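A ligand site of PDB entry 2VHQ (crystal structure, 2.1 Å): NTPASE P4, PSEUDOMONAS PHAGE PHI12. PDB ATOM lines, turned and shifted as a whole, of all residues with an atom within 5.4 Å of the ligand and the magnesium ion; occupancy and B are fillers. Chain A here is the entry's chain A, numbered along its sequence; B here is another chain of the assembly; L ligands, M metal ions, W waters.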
ATOM      1  N   ASN A 133     -15.558 -20.602  22.754  1.00  0.00           N
ATOM      2  CA  ASN A 133     -16.464 -21.456  21.978  1.00  0.00           C
ATOM      3  C   ASN A 133     -15.813 -22.501  21.091  1.00  0.00           C
ATOM      4  O   ASN A 133     -16.462 -23.502  20.759  1.00  0.00           O
ATOM      5  CB  ASN A 133     -17.431 -20.597  21.143  1.00  0.00           C
ATOM      6  CG  ASN A 133     -18.609 -20.081  21.961  1.00  0.00           C
ATOM      7  OD1 ASN A 133     -18.805 -20.485  23.111  1.00  0.00           O
ATOM      8  ND2 ASN A 133     -19.403 -19.201  21.360  1.00  0.00           N
ATOM      9  N   SER A 134     -14.543 -22.286  20.726  1.00  0.00           N
ATOM     10  CA  SER A 134     -13.820 -23.215  19.835  1.00  0.00           C
ATOM     11  C   SER A 134     -13.660 -24.609  20.483  1.00  0.00           C
ATOM     12  O   SER A 134     -13.328 -24.723  21.654  1.00  0.00           O
ATOM     13  CB  SER A 134     -12.466 -22.602  19.422  1.00  0.00           C
ATOM     14  OG  SER A 134     -12.627 -21.275  18.903  1.00  0.00           O
ATOM     15  N   GLY A 135     -13.932 -25.667  19.722  1.00  0.00           N
ATOM     16  CA  GLY A 135     -14.035 -27.045  20.229  1.00  0.00           C
ATOM     17  C   GLY A 135     -12.714 -27.809  20.162  1.00  0.00           C
ATOM     18  O   GLY A 135     -12.095 -27.918  19.091  1.00  0.00           O
ATOM     19  N   LYS A 136     -12.304 -28.367  21.292  1.00  0.00           N
ATOM     20  CA  LYS A 136     -10.969 -28.935  21.402  1.00  0.00           C
ATOM     21  C   LYS A 136     -10.832 -30.256  20.651  1.00  0.00           C
ATOM     22  O   LYS A 136      -9.882 -30.470  19.939  1.00  0.00           O
ATOM     23  CB  LYS A 136     -10.565 -29.070  22.881  1.00  0.00           C
ATOM     24  CG  LYS A 136     -10.435 -27.698  23.553  1.00  0.00           C
ATOM     25  CD  LYS A 136     -10.045 -27.831  25.005  1.00  0.00           C
ATOM     26  CE  LYS A 136     -10.091 -26.472  25.752  1.00  0.00           C
ATOM     27  NZ  LYS A 136     -11.436 -26.165  26.325  1.00  0.00           N
ATOM     28  N   THR A 137     -11.817 -31.140  20.794  1.00  0.00           N
ATOM     29  CA  THR A 137     -11.774 -32.454  20.158  1.00  0.00           C
ATOM     30  C   THR A 137     -11.683 -32.386  18.615  1.00  0.00           C
ATOM     31  O   THR A 137     -10.849 -33.083  18.030  1.00  0.00           O
ATOM     32  CB  THR A 137     -12.957 -33.307  20.596  1.00  0.00           C
ATOM     33  OG1 THR A 137     -12.875 -33.497  22.011  1.00  0.00           O
ATOM     34  CG2 THR A 137     -12.960 -34.693  19.920  1.00  0.00           C
ATOM     35  N   PRO A 138     -12.542 -31.576  17.959  1.00  0.00           N
ATOM     36  CA  PRO A 138     -12.344 -31.421  16.516  1.00  0.00           C
ATOM     37  C   PRO A 138     -10.949 -30.959  16.136  1.00  0.00           C
ATOM     38  O   PRO A 138     -10.377 -31.451  15.150  1.00  0.00           O
ATOM     39  CB  PRO A 138     -13.403 -30.372  16.136  1.00  0.00           C
ATOM     40  CG  PRO A 138     -14.507 -30.642  17.136  1.00  0.00           C
ATOM     41  CD  PRO A 138     -13.756 -30.877  18.411  1.00  0.00           C
ATOM     42  N   GLU A 160     -14.188 -40.455  28.747  1.00  0.00           N
ATOM     43  CA  GLU A 160     -15.314 -39.648  28.291  1.00  0.00           C
ATOM     44  C   GLU A 160     -16.543 -40.556  28.339  1.00  0.00           C
ATOM     45  O   GLU A 160     -16.407 -41.747  28.179  1.00  0.00           O
ATOM     46  CB  GLU A 160     -15.093 -39.135  26.868  1.00  0.00           C
ATOM     47  CG  GLU A 160     -13.934 -38.127  26.701  1.00  0.00           C
ATOM     48  CD  GLU A 160     -14.164 -36.807  27.423  1.00  0.00           C
ATOM     49  OE1 GLU A 160     -15.255 -36.221  27.286  1.00  0.00           O
ATOM     50  OE2 GLU A 160     -13.236 -36.336  28.121  1.00  0.00           O
ATOM     51  N   ASP A 189      -7.721 -38.304  23.554  1.00  0.00           N
ATOM     52  CA  ASP A 189      -8.980 -37.698  23.959  1.00  0.00           C
ATOM     53  C   ASP A 189      -9.519 -38.566  25.103  1.00  0.00           C
ATOM     54  O   ASP A 189      -9.995 -39.651  24.855  1.00  0.00           O
ATOM     55  CB  ASP A 189      -9.958 -37.665  22.796  1.00  0.00           C
ATOM     56  CG  ASP A 189     -11.187 -36.794  23.065  1.00  0.00           C
ATOM     57  OD1 ASP A 189     -11.430 -36.367  24.233  1.00  0.00           O
ATOM     58  OD2 ASP A 189     -11.929 -36.539  22.082  1.00  0.00           O
ATOM     59  N   SER A 232      -6.149 -33.060  24.339  1.00  0.00           N
ATOM     60  CA  SER A 232      -7.057 -32.005  24.785  1.00  0.00           C
ATOM     61  C   SER A 232      -7.165 -31.987  26.291  1.00  0.00           C
ATOM     62  O   SER A 232      -7.212 -33.033  26.946  1.00  0.00           O
ATOM     63  CB  SER A 232      -8.462 -32.114  24.178  1.00  0.00           C
ATOM     64  OG  SER A 232      -9.166 -33.226  24.653  1.00  0.00           O
ATOM     65  N   ASN A 234      -9.582 -29.739  28.904  1.00  0.00           N
ATOM     66  CA  ASN A 234     -10.591 -28.756  29.266  1.00  0.00           C
ATOM     67  C   ASN A 234     -10.292 -28.227  30.674  1.00  0.00           C
ATOM     68  O   ASN A 234     -10.230 -28.989  31.633  1.00  0.00           O
ATOM     69  CB  ASN A 234     -12.010 -29.351  29.168  1.00  0.00           C
ATOM     70  CG  ASN A 234     -12.583 -29.250  27.744  1.00  0.00           C
ATOM     71  OD1 ASN A 234     -11.933 -29.621  26.772  1.00  0.00           O
ATOM     72  ND2 ASN A 234     -13.817 -28.779  27.629  1.00  0.00           N
ATOM     73  N   TYR A 288     -15.493 -25.795  10.030  1.00  0.00           N
ATOM     74  CA  TYR A 288     -16.160 -27.087  10.013  1.00  0.00           C
ATOM     75  C   TYR A 288     -16.772 -27.423   8.640  1.00  0.00           C
ATOM     76  O   TYR A 288     -17.265 -26.550   7.929  1.00  0.00           O
ATOM     77  CB  TYR A 288     -17.255 -27.135  11.075  1.00  0.00           C
ATOM     78  CG  TYR A 288     -16.755 -27.103  12.483  1.00  0.00           C
ATOM     79  CD1 TYR A 288     -16.458 -28.262  13.159  1.00  0.00           C
ATOM     80  CD2 TYR A 288     -16.616 -25.896  13.161  1.00  0.00           C
ATOM     81  CE1 TYR A 288     -16.010 -28.250  14.450  1.00  0.00           C
ATOM     82  CE2 TYR A 288     -16.178 -25.865  14.462  1.00  0.00           C
ATOM     83  CZ  TYR A 288     -15.869 -27.046  15.105  1.00  0.00           C
ATOM     84  OH  TYR A 288     -15.415 -27.034  16.382  1.00  0.00           O
ATOM     85  N   GLY A 289     -16.727 -28.698   8.293  1.00  0.00           N
ATOM     86  CA  GLY A 289     -17.461 -29.241   7.156  1.00  0.00           C
ATOM     87  C   GLY A 289     -18.553 -30.112   7.728  1.00  0.00           C
ATOM     88  O   GLY A 289     -19.021 -29.888   8.840  1.00  0.00           O
ATOM     89  N   SER A 292     -19.102 -32.337  11.646  1.00  0.00           N
ATOM     90  CA  SER A 292     -18.168 -31.661  12.534  1.00  0.00           C
ATOM     91  C   SER A 292     -16.670 -31.884  12.232  1.00  0.00           C
ATOM     92  O   SER A 292     -15.830 -31.609  13.095  1.00  0.00           O
ATOM     93  CB  SER A 292     -18.489 -32.021  13.991  1.00  0.00           C
ATOM     94  OG  SER A 292     -19.717 -31.394  14.401  1.00  0.00           O
ATOM     95  N   ARG B 251     -20.453 -31.834  34.202  1.00  0.00           N
ATOM     96  CA  ARG B 251     -19.779 -31.195  33.083  1.00  0.00           C
ATOM     97  C   ARG B 251     -19.095 -32.257  32.231  1.00  0.00           C
ATOM     98  O   ARG B 251     -19.280 -32.314  31.022  1.00  0.00           O
ATOM     99  CB  ARG B 251     -18.757 -30.196  33.652  1.00  0.00           C
ATOM    100  CG  ARG B 251     -18.124 -29.256  32.673  1.00  0.00           C
ATOM    101  CD  ARG B 251     -17.024 -28.447  33.380  1.00  0.00           C
ATOM    102  NE  ARG B 251     -17.572 -27.648  34.478  1.00  0.00           N
ATOM    103  CZ  ARG B 251     -18.168 -26.469  34.330  1.00  0.00           C
ATOM    104  NH1 ARG B 251     -18.294 -25.929  33.121  1.00  0.00           N
ATOM    105  NH2 ARG B 251     -18.640 -25.821  35.391  1.00  0.00           N
ATOM    106  N   ARG B 272     -25.066 -34.384  24.495  1.00  0.00           N
ATOM    107  CA  ARG B 272     -23.915 -34.659  23.649  1.00  0.00           C
ATOM    108  C   ARG B 272     -24.363 -35.686  22.652  1.00  0.00           C
ATOM    109  O   ARG B 272     -24.948 -36.721  23.036  1.00  0.00           O
ATOM    110  CB  ARG B 272     -22.724 -35.167  24.469  1.00  0.00           C
ATOM    111  CG  ARG B 272     -22.255 -34.199  25.528  1.00  0.00           C
ATOM    112  CD  ARG B 272     -21.172 -34.792  26.435  1.00  0.00           C
ATOM    113  NE  ARG B 272     -19.955 -35.108  25.684  1.00  0.00           N
ATOM    114  CZ  ARG B 272     -18.728 -35.128  26.208  1.00  0.00           C
ATOM    115  NH1 ARG B 272     -18.537 -34.889  27.501  1.00  0.00           N
ATOM    116  NH2 ARG B 272     -17.700 -35.421  25.428  1.00  0.00           N
ATOM    117  N   GLY B 274     -22.323 -37.016  20.291  1.00  0.00           N
ATOM    118  CA  GLY B 274     -21.237 -37.917  19.966  1.00  0.00           C
ATOM    119  C   GLY B 274     -19.903 -37.212  20.060  1.00  0.00           C
ATOM    120  O   GLY B 274     -19.825 -36.012  20.342  1.00  0.00           O
ATOM    121  N   GLY B 276     -16.840 -35.242  19.408  1.00  0.00           N
ATOM    122  CA  GLY B 276     -16.603 -34.067  18.576  1.00  0.00           C
ATOM    123  C   GLY B 276     -17.809 -33.450  17.901  1.00  0.00           C
ATOM    124  O   GLY B 276     -17.671 -32.519  17.117  1.00  0.00           O
ATOM    125  N   LEU B 277     -19.017 -33.963  18.173  1.00  0.00           N
ATOM    126  CA  LEU B 277     -20.205 -33.452  17.529  1.00  0.00           C
ATOM    127  C   LEU B 277     -20.815 -32.325  18.378  1.00  0.00           C
ATOM    128  O   LEU B 277     -20.369 -32.062  19.505  1.00  0.00           O
ATOM    129  CB  LEU B 277     -21.222 -34.575  17.290  1.00  0.00           C
ATOM    130  CG  LEU B 277     -20.750 -35.790  16.487  1.00  0.00           C
ATOM    131  CD1 LEU B 277     -21.834 -36.835  16.433  1.00  0.00           C
ATOM    132  CD2 LEU B 277     -20.306 -35.420  15.054  1.00  0.00           C
ATOM    133  N   GLN B 278     -21.821 -31.653  17.819  1.00  0.00           N
ATOM    134  CA  GLN B 278     -22.454 -30.548  18.561  1.00  0.00           C
ATOM    135  C   GLN B 278     -23.362 -31.024  19.700  1.00  0.00           C
ATOM    136  O   GLN B 278     -23.972 -32.072  19.642  1.00  0.00           O
ATOM    137  CB  GLN B 278     -23.217 -29.597  17.630  1.00  0.00           C
ATOM    138  CG  GLN B 278     -22.375 -28.364  17.267  1.00  0.00           C
ATOM    139  CD  GLN B 278     -22.889 -27.615  16.064  1.00  0.00           C
ATOM    140  OE1 GLN B 278     -23.463 -28.195  15.149  1.00  0.00           O
ATOM    141  NE2 GLN B 278     -22.674 -26.297  16.048  1.00  0.00           N
ATOM    142  N   ARG B 279     -23.369 -30.244  20.758  1.00  0.00           N
ATOM    143  CA  ARG B 279     -24.307 -30.409  21.852  1.00  0.00           C
ATOM    144  C   ARG B 279     -25.650 -29.800  21.435  1.00  0.00           C
ATOM    145  O   ARG B 279     -25.671 -28.684  20.912  1.00  0.00           O
ATOM    146  CB  ARG B 279     -23.769 -29.683  23.077  1.00  0.00           C
ATOM    147  CG  ARG B 279     -23.957 -30.426  24.356  1.00  0.00           C
ATOM    148  CD  ARG B 279     -22.807 -30.150  25.302  1.00  0.00           C
ATOM    149  NE  ARG B 279     -21.529 -30.669  24.790  1.00  0.00           N
ATOM    150  CZ  ARG B 279     -20.431 -30.794  25.538  1.00  0.00           C
ATOM    151  NH1 ARG B 279     -20.447 -30.461  26.825  1.00  0.00           N
ATOM    152  NH2 ARG B 279     -19.312 -31.270  25.001  1.00  0.00           N
ATOM    153  N   ILE B 316     -26.243 -25.687  21.466  1.00  0.00           N
ATOM    154  CA  ILE B 316     -25.743 -24.805  22.523  1.00  0.00           C
ATOM    155  C   ILE B 316     -24.234 -24.640  22.350  1.00  0.00           C
ATOM    156  O   ILE B 316     -23.547 -25.554  21.892  1.00  0.00           O
ATOM    157  CB  ILE B 316     -26.114 -25.334  23.933  1.00  0.00           C
ATOM    158  CG1 ILE B 316     -25.967 -24.235  24.979  1.00  0.00           C
ATOM    159  CG2 ILE B 316     -25.262 -26.544  24.294  1.00  0.00           C
ATOM    160  CD1 ILE B 316     -26.752 -24.487  26.255  1.00  0.00           C
ATOM    161  N   LYS B 317     -23.713 -23.471  22.736  1.00  0.00           N
ATOM    162  CA  LYS B 317     -22.400 -23.005  22.256  1.00  0.00           C
ATOM    163  C   LYS B 317     -21.268 -22.936  23.273  1.00  0.00           C
ATOM    164  O   LYS B 317     -20.540 -21.949  23.310  1.00  0.00           O
ATOM    165  CB  LYS B 317     -22.559 -21.618  21.631  1.00  0.00           C
ATOM    166  CG  LYS B 317     -23.418 -21.592  20.377  1.00  0.00           C
ATOM    167  CD  LYS B 317     -22.898 -20.586  19.361  1.00  0.00           C
ATOM    168  CE  LYS B 317     -23.705 -20.666  18.069  1.00  0.00           C
ATOM    169  NZ  LYS B 317     -23.545 -19.439  17.244  1.00  0.00           N
ATOM    170  N   ASN B 318     -21.094 -23.955  24.097  1.00  0.00           N
ATOM    171  CA  ASN B 318     -19.897 -24.064  24.967  1.00  0.00           C
ATOM    172  C   ASN B 318     -19.769 -22.967  26.044  1.00  0.00           C
ATOM    173  O   ASN B 318     -19.422 -23.279  27.193  1.00  0.00           O
ATOM    174  CB  ASN B 318     -18.618 -24.144  24.108  1.00  0.00           C
ATOM    175  CG  ASN B 318     -17.625 -25.163  24.629  1.00  0.00           C
ATOM    176  OD1 ASN B 318     -16.976 -24.956  25.654  1.00  0.00           O
ATOM    177  ND2 ASN B 318     -17.487 -26.279  23.915  1.00  0.00           N
HETATM  178  P1  LIG L   1     -15.382 -31.429  26.185  1.00  0.00           P
HETATM  179  O1  LIG L   1     -15.567 -32.706  25.400  1.00  0.00           O
HETATM  180  O2  LIG L   1     -16.671 -30.810  26.677  1.00  0.00           O
HETATM  181  O3  LIG L   1     -14.323 -31.641  27.238  1.00  0.00           O
HETATM  182  P2  LIG L   1     -15.028 -29.979  23.634  1.00  0.00           P
HETATM  183  O4  LIG L   1     -15.158 -28.497  23.429  1.00  0.00           O
HETATM  184  O5  LIG L   1     -14.010 -30.735  22.811  1.00  0.00           O
HETATM  185  O6  LIG L   1     -14.754 -30.234  25.232  1.00  0.00           O
HETATM  186  P3  LIG L   1     -16.628 -31.975  22.526  1.00  0.00           P
HETATM  187  O7  LIG L   1     -18.110 -32.262  22.430  1.00  0.00           O
HETATM  188  O8  LIG L   1     -15.719 -33.105  22.955  1.00  0.00           O
HETATM  189  O9  LIG L   1     -16.437 -30.707  23.466  1.00  0.00           O
HETATM  190  O10 LIG L   1     -16.142 -31.335  21.129  1.00  0.00           O
HETATM  191  C1  LIG L   1     -17.082 -30.941  20.136  1.00  0.00           C
HETATM  192  C2  LIG L   1     -17.411 -29.472  20.293  1.00  0.00           C
HETATM  193  O11 LIG L   1     -16.926 -28.734  19.161  1.00  0.00           O
HETATM  194  C3  LIG L   1     -18.912 -29.185  20.358  1.00  0.00           C
HETATM  195  O12 LIG L   1     -19.440 -29.320  21.686  1.00  0.00           O
HETATM  196  C4  LIG L   1     -18.980 -27.781  19.813  1.00  0.00           C
HETATM  197  O13 LIG L   1     -18.640 -26.865  20.861  1.00  0.00           O
HETATM  198  C5  LIG L   1     -17.901 -27.758  18.754  1.00  0.00           C
HETATM  199  N1  LIG L   1     -18.473 -28.156  17.458  1.00  0.00           N
HETATM  200  C6  LIG L   1     -18.650 -29.415  17.032  1.00  0.00           C
HETATM  201  N2  LIG L   1     -19.198 -29.429  15.794  1.00  0.00           N
HETATM  202  C7  LIG L   1     -19.395 -28.156  15.436  1.00  0.00           C
HETATM  203  C8  LIG L   1     -19.957 -27.481  14.260  1.00  0.00           C
HETATM  204  N3  LIG L   1     -20.413 -28.220  13.226  1.00  0.00           N
HETATM  205  N4  LIG L   1     -19.984 -26.141  14.249  1.00  0.00           N
HETATM  206  C9  LIG L   1     -19.525 -25.412  15.285  1.00  0.00           C
HETATM  207  N5  LIG L   1     -19.006 -25.970  16.404  1.00  0.00           N
HETATM  208  C10 LIG L   1     -18.924 -27.320  16.528  1.00  0.00           C
HETATM  209 MG    MG M   1     -14.242 -32.728  23.829  1.00  0.00          MG
HETATM  210  O   HOH W   1     -12.790 -33.632  28.087  1.00  0.00           O
HETATM  211  O   HOH W   2     -16.447 -35.405  22.144  1.00  0.00           O
HETATM  212  O   HOH W   3     -19.395 -34.642  22.868  1.00  0.00           O
HETATM  213  O   HOH W   4     -20.638 -29.923  11.056  1.00  0.00           O
HETATM  214  O   HOH W   5     -22.207 -27.277  20.819  1.00  0.00           O
HETATM  215  O   HOH W   6     -21.329 -25.976  10.937  1.00  0.00           O
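The backbone NH (N) of Thr 137 lies close to an oxygen (O5) of the ligand (3.0 Å). A nitrogen (N2) of the ligand is in hydrogen-bond range of the side-chain hydroxyl of Ser 292, at 2.5 Å. The side-chain amide nitrogen of Asn 234 lies within hydrogen-bond range of an oxygen (O3) of the ligand, 2.9 Å away. An oxygen (O7) of the ligand lies within salt-bridge range of the guanidinium group of Arg 279 of chain B (3.0 Å). The side-chain amide nitrogen of Gln 278 of chain B sits at hydrogen-bond distance from a nitrogen (N4) of the ligand. ND2 of Asn 318 of chain B is in hydrogen-bond range of O4 of the ligand (3.3 Å). N of Lys 136 lies close to O5 of the ligand, 3.3 Å away. NH2 of Arg 272 of chain B sits close to O1 of the ligand, 3.5 Å away.
The side-chain hydroxyl of Thr 137 sits close to the side-chain carboxylate of Asp 189. The backbone NH (N) of Ile 316 of chain B lies within hydrogen-bond range of the backbone carbonyl oxygen (O) of Arg 279 of chain B (3.1 Å). The guanidinium group (NH2) of Arg 272 of chain B lies within salt-bridge range of the side-chain carboxylate (OE1) of Glu 160 (3.2 Å).
OH of Tyr 288 sits close to N1 of the ligand, 3.4 Å away. Gly 135 touches the ligand. Pro 138 touches the ligand (CD to O10, 3.6 Å). Gly 276 of chain B touches the ligand (O to C6, 3.3 Å). Leu 277 of chain B touches the ligand (O to C3, 3.3 Å). Hydrophobic or aromatic side chains that line the ligand: Pro 138 and Tyr 288. Within 4 Å of the ligand: Gly 135, Lys 136, Thr 137, Pro 138, Asn 234, Tyr 288, Ser 292, Arg 272 of chain B, Gly 276 of chain B, Leu 277 of chain B, Gln 278 of chain B, Arg 279 of chain B and Asn 318 of chain B.
One residue has an atom within 4 Å of the magnesium ion: Thr 137. The nearest printed residue that does not touch the magnesium ion is Asp 189 (4.6 Å).
The magnesium ion is bound by O8 of the ligand (1.8 Å), O1 of the ligand (2.1 Å), O5 of the ligand (2.2 Å) and OG1 of Thr 137 (2.4 Å). The magnesium ion has four donor atoms within binding distance.
Water W1 lies within hydrogen-bond range of an oxygen (O3) of the ligand (2.7 Å) and the side-chain carboxylate (OE2) of Glu 160 (2.7 Å). Water W3 lies within hydrogen-bond range of an oxygen (O7) of the ligand, the backbone carbonyl oxygen of Gly 274 of chain B and the guanidinium group of Arg 272 of chain B. Water W4 lies within hydrogen-bond range of the backbone carbonyl oxygen of Gly 289 (2.7 Å), a nitrogen (N3) of the ligand (2.8 Å) and the backbone NH of Ser 292 (2.9 Å). Water W5 lies within hydrogen-bond range of the backbone carbonyl oxygen (O) of Ile 316 of chain B (2.4 Å) and the backbone NH (N) of Arg 279 of chain B (3.2 Å).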
